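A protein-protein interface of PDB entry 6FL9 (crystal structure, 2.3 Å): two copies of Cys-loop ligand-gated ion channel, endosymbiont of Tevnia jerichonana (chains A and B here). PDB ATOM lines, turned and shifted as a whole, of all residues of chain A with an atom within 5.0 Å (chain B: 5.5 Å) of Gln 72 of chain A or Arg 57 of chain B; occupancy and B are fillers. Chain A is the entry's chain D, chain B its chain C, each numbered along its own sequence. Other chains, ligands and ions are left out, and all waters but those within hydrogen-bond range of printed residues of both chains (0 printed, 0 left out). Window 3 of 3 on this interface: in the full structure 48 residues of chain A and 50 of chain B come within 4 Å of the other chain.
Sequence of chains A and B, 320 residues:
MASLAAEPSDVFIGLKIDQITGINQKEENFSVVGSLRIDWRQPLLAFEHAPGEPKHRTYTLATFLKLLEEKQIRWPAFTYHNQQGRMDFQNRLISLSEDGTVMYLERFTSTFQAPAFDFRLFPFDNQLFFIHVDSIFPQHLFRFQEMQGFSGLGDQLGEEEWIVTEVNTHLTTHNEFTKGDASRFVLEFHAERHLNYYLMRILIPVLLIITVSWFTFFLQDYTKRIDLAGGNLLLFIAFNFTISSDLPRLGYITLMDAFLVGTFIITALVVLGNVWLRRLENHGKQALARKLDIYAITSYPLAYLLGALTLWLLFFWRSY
NE of Arg 57 of chain B is in hydrogen-bond range of OE1 of Gln 72 of chain A.
N of Arg 57 of chain B sits at hydrogen-bond distance from O of Leu 96 of chain B. The backbone carbonyl oxygen (O) of Ile 94 of chain B lies within hydrogen-bond range of the backbone NH (N) of Tyr 59 of chain B (2.8 Å). N of Ile 73 of chain A sits at hydrogen-bond distance from O of Leu 68 of chain A.
Among the printed residues, pairs that only touch across the chains: Arg 74 of chain A with Thr 58 of chain B (2.8 Å), Arg 74 of chain A with His 56 of chain B (3.5 Å), Ile 73 of chain A with Thr 58 of chain B (3.7 Å), Gln 72 of chain A with Pro 54 of chain B (3.8 Å), Arg 74 of chain A with Ser 95 of chain B (3.8 Å) and Glu 69 of chain A with Tyr 59 of chain B (3.9 Å).
Gln 72 of chain A touches just these residues of chain B: Pro 54 (3.8 Å) and Arg 57 (3.4 Å). Arg 57 of chain B touches just one residue of chain A: Gln 72 (3.4 Å). Printed residues of chain A within 4 Å of Thr 58 of chain B: Ile 73 and Arg 74. Of the printed residues of chain B, Ile 73 of chain A touches Thr 58 (3.7 Å). Printed residues of chain B within 4 Å of Arg 74 of chain A: His 56, Thr 58 and Ser 95. Leu 68 of chain A touches none of the printed residues of chain B. The nearest printed residue of chain A that does not touch Arg 57 of chain B is Arg 74 of chain A (5.4 Å).
Of the 7 printed residues of chain A, 4 touch a printed residue of chain B. Of the 13 printed residues of chain B, 6 touch a printed residue of chain A. Hydrophobic or aromatic side chains of chain B within 4 Å of the printed part of chain A: Pro 54 and His 56. Along chain B the printed residues that touch a printed residue of chain A span positions 54 to 95. Among the printed residues, 7 pairs touch across the chains.
No position is printed for both chains. Of the 7 pairs that touch across the chains among the printed residues, none has its exchanged pair printed and touching as well.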
ATOM      1  N   LEU A  68      34.683  11.450  -9.133  1.00  0.00           N
ATOM      2  CA  LEU A  68      34.549  10.678  -7.893  1.00  0.00           C
ATOM      3  C   LEU A  68      33.201  10.905  -7.226  1.00  0.00           C
ATOM      4  O   LEU A  68      32.608   9.947  -6.728  1.00  0.00           O
ATOM      5  CB  LEU A  68      35.659  11.005  -6.890  1.00  0.00           C
ATOM      6  CG  LEU A  68      37.069  10.622  -7.274  1.00  0.00           C
ATOM      7  CD1 LEU A  68      38.065  11.457  -6.496  1.00  0.00           C
ATOM      8  CD2 LEU A  68      37.318   9.140  -7.050  1.00  0.00           C
ATOM      9  N   GLU A  69      32.724  12.166  -7.203  1.00  0.00           N
ATOM     10  CA  GLU A  69      31.440  12.534  -6.594  1.00  0.00           C
ATOM     11  C   GLU A  69      30.290  11.859  -7.317  1.00  0.00           C
ATOM     12  O   GLU A  69      29.350  11.362  -6.677  1.00  0.00           O
ATOM     13  CB  GLU A  69      31.260  14.057  -6.604  1.00  0.00           C
ATOM     14  CG  GLU A  69      32.195  14.796  -5.667  1.00  0.00           C
ATOM     15  CD  GLU A  69      32.331  16.284  -5.929  1.00  0.00           C
ATOM     16  OE1 GLU A  69      32.353  16.695  -7.111  1.00  0.00           O
ATOM     17  OE2 GLU A  69      32.470  17.039  -4.940  1.00  0.00           O
ATOM     18  N   GLU A  70      30.393  11.824  -8.666  1.00  0.00           N
ATOM     19  CA  GLU A  70      29.446  11.193  -9.592  1.00  0.00           C
ATOM     20  C   GLU A  70      29.374   9.703  -9.301  1.00  0.00           C
ATOM     21  O   GLU A  70      28.285   9.186  -9.064  1.00  0.00           O
ATOM     22  CB  GLU A  70      29.924  11.390 -11.040  1.00  0.00           C
ATOM     23  CG  GLU A  70      28.986  12.190 -11.921  1.00  0.00           C
ATOM     24  CD  GLU A  70      29.607  12.537 -13.258  1.00  0.00           C
ATOM     25  OE1 GLU A  70      29.391  11.769 -14.223  1.00  0.00           O
ATOM     26  OE2 GLU A  70      30.357  13.541 -13.328  1.00  0.00           O
ATOM     27  N   LYS A  71      30.540   9.022  -9.293  1.00  0.00           N
ATOM     28  CA  LYS A  71      30.643   7.588  -9.036  1.00  0.00           C
ATOM     29  C   LYS A  71      30.410   7.238  -7.552  1.00  0.00           C
ATOM     30  O   LYS A  71      30.464   6.057  -7.203  1.00  0.00           O
ATOM     31  CB  LYS A  71      31.989   7.030  -9.556  1.00  0.00           C
ATOM     32  CG  LYS A  71      32.209   7.169 -11.062  1.00  0.00           C
ATOM     33  CD  LYS A  71      33.294   6.216 -11.584  1.00  0.00           C
ATOM     34  CE  LYS A  71      33.088   5.857 -13.043  1.00  0.00           C
ATOM     35  NZ  LYS A  71      33.515   4.460 -13.359  1.00  0.00           N
ATOM     36  N   GLN A  72      30.123   8.261  -6.689  1.00  0.00           N
ATOM     37  CA  GLN A  72      29.890   8.118  -5.238  1.00  0.00           C
ATOM     38  C   GLN A  72      31.098   7.462  -4.500  1.00  0.00           C
ATOM     39  O   GLN A  72      30.911   6.713  -3.538  1.00  0.00           O
ATOM     40  CB  GLN A  72      28.566   7.377  -4.937  1.00  0.00           C
ATOM     41  CG  GLN A  72      27.337   8.266  -4.948  1.00  0.00           C
ATOM     42  CD  GLN A  72      26.047   7.465  -4.869  1.00  0.00           C
ATOM     43  OE1 GLN A  72      25.717   6.827  -3.857  1.00  0.00           O
ATOM     44  NE2 GLN A  72      25.280   7.487  -5.947  1.00  0.00           N
ATOM     45  N   ILE A  73      32.331   7.761  -4.964  1.00  0.00           N
ATOM     46  CA  ILE A  73      33.582   7.261  -4.393  1.00  0.00           C
ATOM     47  C   ILE A  73      34.225   8.320  -3.453  1.00  0.00           C
ATOM     48  O   ILE A  73      34.209   9.523  -3.739  1.00  0.00           O
ATOM     49  CB  ILE A  73      34.577   6.772  -5.495  1.00  0.00           C
ATOM     50  CG1 ILE A  73      33.953   5.662  -6.356  1.00  0.00           C
ATOM     51  CG2 ILE A  73      35.950   6.323  -4.898  1.00  0.00           C
ATOM     52  CD1 ILE A  73      34.663   5.410  -7.669  1.00  0.00           C
ATOM     53  N   ARG A  74      34.764   7.833  -2.331  1.00  0.00           N
ATOM     54  CA  ARG A  74      35.417   8.606  -1.296  1.00  0.00           C
ATOM     55  C   ARG A  74      36.916   8.533  -1.554  1.00  0.00           C
ATOM     56  O   ARG A  74      37.495   7.444  -1.632  1.00  0.00           O
ATOM     57  CB  ARG A  74      35.060   8.043   0.085  1.00  0.00           C
ATOM     58  CG  ARG A  74      35.651   8.807   1.247  1.00  0.00           C
ATOM     59  CD  ARG A  74      35.658   8.025   2.548  1.00  0.00           C
ATOM     60  NE  ARG A  74      34.447   7.211   2.751  1.00  0.00           N
ATOM     61  CZ  ARG A  74      33.340   7.648   3.357  1.00  0.00           C
ATOM     62  NH1 ARG A  74      33.263   8.906   3.798  1.00  0.00           N
ATOM     63  NH2 ARG A  74      32.301   6.841   3.513  1.00  0.00           N
ATOM     64  N   PHE B  47      18.970  10.325   2.074  1.00  0.00           N
ATOM     65  CA  PHE B  47      18.946   9.620   0.794  1.00  0.00           C
ATOM     66  C   PHE B  47      18.762   8.114   0.925  1.00  0.00           C
ATOM     67  O   PHE B  47      18.976   7.535   1.994  1.00  0.00           O
ATOM     68  CB  PHE B  47      20.207   9.965  -0.047  1.00  0.00           C
ATOM     69  CG  PHE B  47      21.529   9.635   0.577  1.00  0.00           C
ATOM     70  CD1 PHE B  47      22.038   8.337   0.523  1.00  0.00           C
ATOM     71  CD2 PHE B  47      22.268  10.615   1.226  1.00  0.00           C
ATOM     72  CE1 PHE B  47      23.250   8.021   1.132  1.00  0.00           C
ATOM     73  CE2 PHE B  47      23.496  10.313   1.814  1.00  0.00           C
ATOM     74  CZ  PHE B  47      23.994   9.029   1.748  1.00  0.00           C
ATOM     75  N   GLU B  48      18.326   7.490  -0.165  1.00  0.00           N
ATOM     76  CA  GLU B  48      18.161   6.064  -0.230  1.00  0.00           C
ATOM     77  C   GLU B  48      19.416   5.472  -0.868  1.00  0.00           C
ATOM     78  O   GLU B  48      20.104   6.138  -1.642  1.00  0.00           O
ATOM     79  CB  GLU B  48      16.906   5.705  -1.012  1.00  0.00           C
ATOM     80  CG  GLU B  48      15.611   5.924  -0.238  1.00  0.00           C
ATOM     81  CD  GLU B  48      14.342   5.475  -0.940  1.00  0.00           C
ATOM     82  OE1 GLU B  48      14.283   4.299  -1.368  1.00  0.00           O
ATOM     83  OE2 GLU B  48      13.390   6.288  -1.019  1.00  0.00           O
ATOM     84  N   GLU B  53      25.816  -0.461  -1.905  1.00  0.00           N
ATOM     85  CA  GLU B  53      26.062   0.948  -2.198  1.00  0.00           C
ATOM     86  C   GLU B  53      26.346   1.724  -0.886  1.00  0.00           C
ATOM     87  O   GLU B  53      25.724   1.409   0.136  1.00  0.00           O
ATOM     88  CB  GLU B  53      24.864   1.556  -2.934  1.00  0.00           C
ATOM     89  CG  GLU B  53      24.887   1.336  -4.430  1.00  0.00           C
ATOM     90  CD  GLU B  53      23.738   1.985  -5.182  1.00  0.00           C
ATOM     91  OE1 GLU B  53      23.436   3.179  -4.940  1.00  0.00           O
ATOM     92  OE2 GLU B  53      23.161   1.297  -6.053  1.00  0.00           O
ATOM     93  N   PRO B  54      27.254   2.719  -0.898  1.00  0.00           N
ATOM     94  CA  PRO B  54      27.593   3.445   0.345  1.00  0.00           C
ATOM     95  C   PRO B  54      26.494   4.259   1.019  1.00  0.00           C
ATOM     96  O   PRO B  54      25.681   4.935   0.392  1.00  0.00           O
ATOM     97  CB  PRO B  54      28.752   4.368  -0.064  1.00  0.00           C
ATOM     98  CG  PRO B  54      28.691   4.474  -1.505  1.00  0.00           C
ATOM     99  CD  PRO B  54      28.109   3.163  -2.012  1.00  0.00           C
ATOM    100  N   LYS B  55      26.539   4.210   2.332  1.00  0.00           N
ATOM    101  CA  LYS B  55      25.676   4.883   3.280  1.00  0.00           C
ATOM    102  C   LYS B  55      26.173   6.314   3.573  1.00  0.00           C
ATOM    103  O   LYS B  55      25.448   7.059   4.229  1.00  0.00           O
ATOM    104  CB  LYS B  55      25.716   4.071   4.576  1.00  0.00           C
ATOM    105  CG  LYS B  55      24.470   4.168   5.434  1.00  0.00           C
ATOM    106  CD  LYS B  55      24.666   3.417   6.735  1.00  0.00           C
ATOM    107  CE  LYS B  55      25.462   4.173   7.754  1.00  0.00           C
ATOM    108  NZ  LYS B  55      24.619   5.181   8.430  1.00  0.00           N
ATOM    109  N   HIS B  56      27.405   6.689   3.125  1.00  0.00           N
ATOM    110  CA  HIS B  56      28.007   8.021   3.316  1.00  0.00           C
ATOM    111  C   HIS B  56      28.572   8.586   2.010  1.00  0.00           C
ATOM    112  O   HIS B  56      29.418   7.956   1.368  1.00  0.00           O
ATOM    113  CB  HIS B  56      29.112   8.010   4.396  1.00  0.00           C
ATOM    114  CG  HIS B  56      28.653   7.569   5.745  1.00  0.00           C
ATOM    115  ND1 HIS B  56      28.012   8.437   6.609  1.00  0.00           N
ATOM    116  CD2 HIS B  56      28.758   6.357   6.338  1.00  0.00           C
ATOM    117  CE1 HIS B  56      27.755   7.733   7.699  1.00  0.00           C
ATOM    118  NE2 HIS B  56      28.185   6.475   7.581  1.00  0.00           N
ATOM    119  N   ARG B  57      28.122   9.799   1.648  1.00  0.00           N
ATOM    120  CA  ARG B  57      28.522  10.520   0.439  1.00  0.00           C
ATOM    121  C   ARG B  57      29.484  11.623   0.789  1.00  0.00           C
ATOM    122  O   ARG B  57      29.194  12.452   1.652  1.00  0.00           O
ATOM    123  CB  ARG B  57      27.294  11.073  -0.316  1.00  0.00           C
ATOM    124  CG  ARG B  57      26.490   9.997  -1.020  1.00  0.00           C
ATOM    125  CD  ARG B  57      25.140  10.477  -1.480  1.00  0.00           C
ATOM    126  NE  ARG B  57      24.378   9.350  -2.010  1.00  0.00           N
ATOM    127  CZ  ARG B  57      23.195   9.459  -2.596  1.00  0.00           C
ATOM    128  NH1 ARG B  57      22.626  10.646  -2.748  1.00  0.00           N
ATOM    129  NH2 ARG B  57      22.572   8.374  -3.046  1.00  0.00           N
ATOM    130  N   THR B  58      30.646  11.622   0.127  1.00  0.00           N
ATOM    131  CA  THR B  58      31.715  12.577   0.377  1.00  0.00           C
ATOM    132  C   THR B  58      31.764  13.640  -0.723  1.00  0.00           C
ATOM    133  O   THR B  58      31.793  13.305  -1.907  1.00  0.00           O
ATOM    134  CB  THR B  58      33.026  11.833   0.629  1.00  0.00           C
ATOM    135  OG1 THR B  58      33.326  11.009  -0.497  1.00  0.00           O
ATOM    136  CG2 THR B  58      32.938  10.956   1.868  1.00  0.00           C
ATOM    137  N   TYR B  59      31.714  14.921  -0.318  1.00  0.00           N
ATOM    138  CA  TYR B  59      31.633  16.055  -1.232  1.00  0.00           C
ATOM    139  C   TYR B  59      32.644  17.160  -0.966  1.00  0.00           C
ATOM    140  O   TYR B  59      32.932  17.496   0.189  1.00  0.00           O
ATOM    141  CB  TYR B  59      30.228  16.695  -1.141  1.00  0.00           C
ATOM    142  CG  TYR B  59      29.068  15.838  -1.590  1.00  0.00           C
ATOM    143  CD1 TYR B  59      28.898  15.507  -2.934  1.00  0.00           C
ATOM    144  CD2 TYR B  59      28.054  15.491  -0.708  1.00  0.00           C
ATOM    145  CE1 TYR B  59      27.796  14.772  -3.370  1.00  0.00           C
ATOM    146  CE2 TYR B  59      26.935  14.761  -1.137  1.00  0.00           C
ATOM    147  CZ  TYR B  59      26.816  14.399  -2.468  1.00  0.00           C
ATOM    148  OH  TYR B  59      25.734  13.681  -2.918  1.00  0.00           O
ATOM    149  N   ILE B  94      32.955  17.750   3.052  1.00  0.00           N
ATOM    150  CA  ILE B  94      31.633  17.370   3.566  1.00  0.00           C
ATOM    151  C   ILE B  94      31.445  15.849   3.485  1.00  0.00           C
ATOM    152  O   ILE B  94      31.726  15.248   2.442  1.00  0.00           O
ATOM    153  CB  ILE B  94      30.520  18.086   2.736  1.00  0.00           C
ATOM    154  CG1 ILE B  94      30.670  19.639   2.771  1.00  0.00           C
ATOM    155  CG2 ILE B  94      29.124  17.644   3.126  1.00  0.00           C
ATOM    156  CD1 ILE B  94      29.871  20.364   3.875  1.00  0.00           C
ATOM    157  N   SER B  95      30.943  15.236   4.578  1.00  0.00           N
ATOM    158  CA  SER B  95      30.504  13.845   4.580  1.00  0.00           C
ATOM    159  C   SER B  95      29.042  13.855   4.994  1.00  0.00           C
ATOM    160  O   SER B  95      28.700  14.380   6.063  1.00  0.00           O
ATOM    161  CB  SER B  95      31.346  12.917   5.461  1.00  0.00           C
ATOM    162  OG  SER B  95      30.959  11.551   5.240  1.00  0.00           O
ATOM    163  N   LEU B  96      28.177  13.367   4.079  1.00  0.00           N
ATOM    164  CA  LEU B  96      26.725  13.312   4.217  1.00  0.00           C
ATOM    165  C   LEU B  96      26.276  11.872   4.376  1.00  0.00           C
ATOM    166  O   LEU B  96      26.537  11.026   3.521  1.00  0.00           O
ATOM    167  CB  LEU B  96      26.036  13.983   3.011  1.00  0.00           C
ATOM    168  CG  LEU B  96      24.506  14.103   3.062  1.00  0.00           C
ATOM    169  CD1 LEU B  96      24.046  15.058   4.149  1.00  0.00           C
ATOM    170  CD2 LEU B  96      23.969  14.577   1.750  1.00  0.00           C
ATOM    171  N   SER B  97      25.626  11.600   5.504  1.00  0.00           N
ATOM    172  CA  SER B  97      25.104  10.293   5.862  1.00  0.00           C
ATOM    173  C   SER B  97      23.704  10.125   5.305  1.00  0.00           C
ATOM    174  O   SER B  97      23.030  11.113   5.006  1.00  0.00           O
ATOM    175  CB  SER B  97      25.054  10.162   7.376  1.00  0.00           C
ATOM    176  OG  SER B  97      24.100  11.061   7.917  1.00  0.00           O
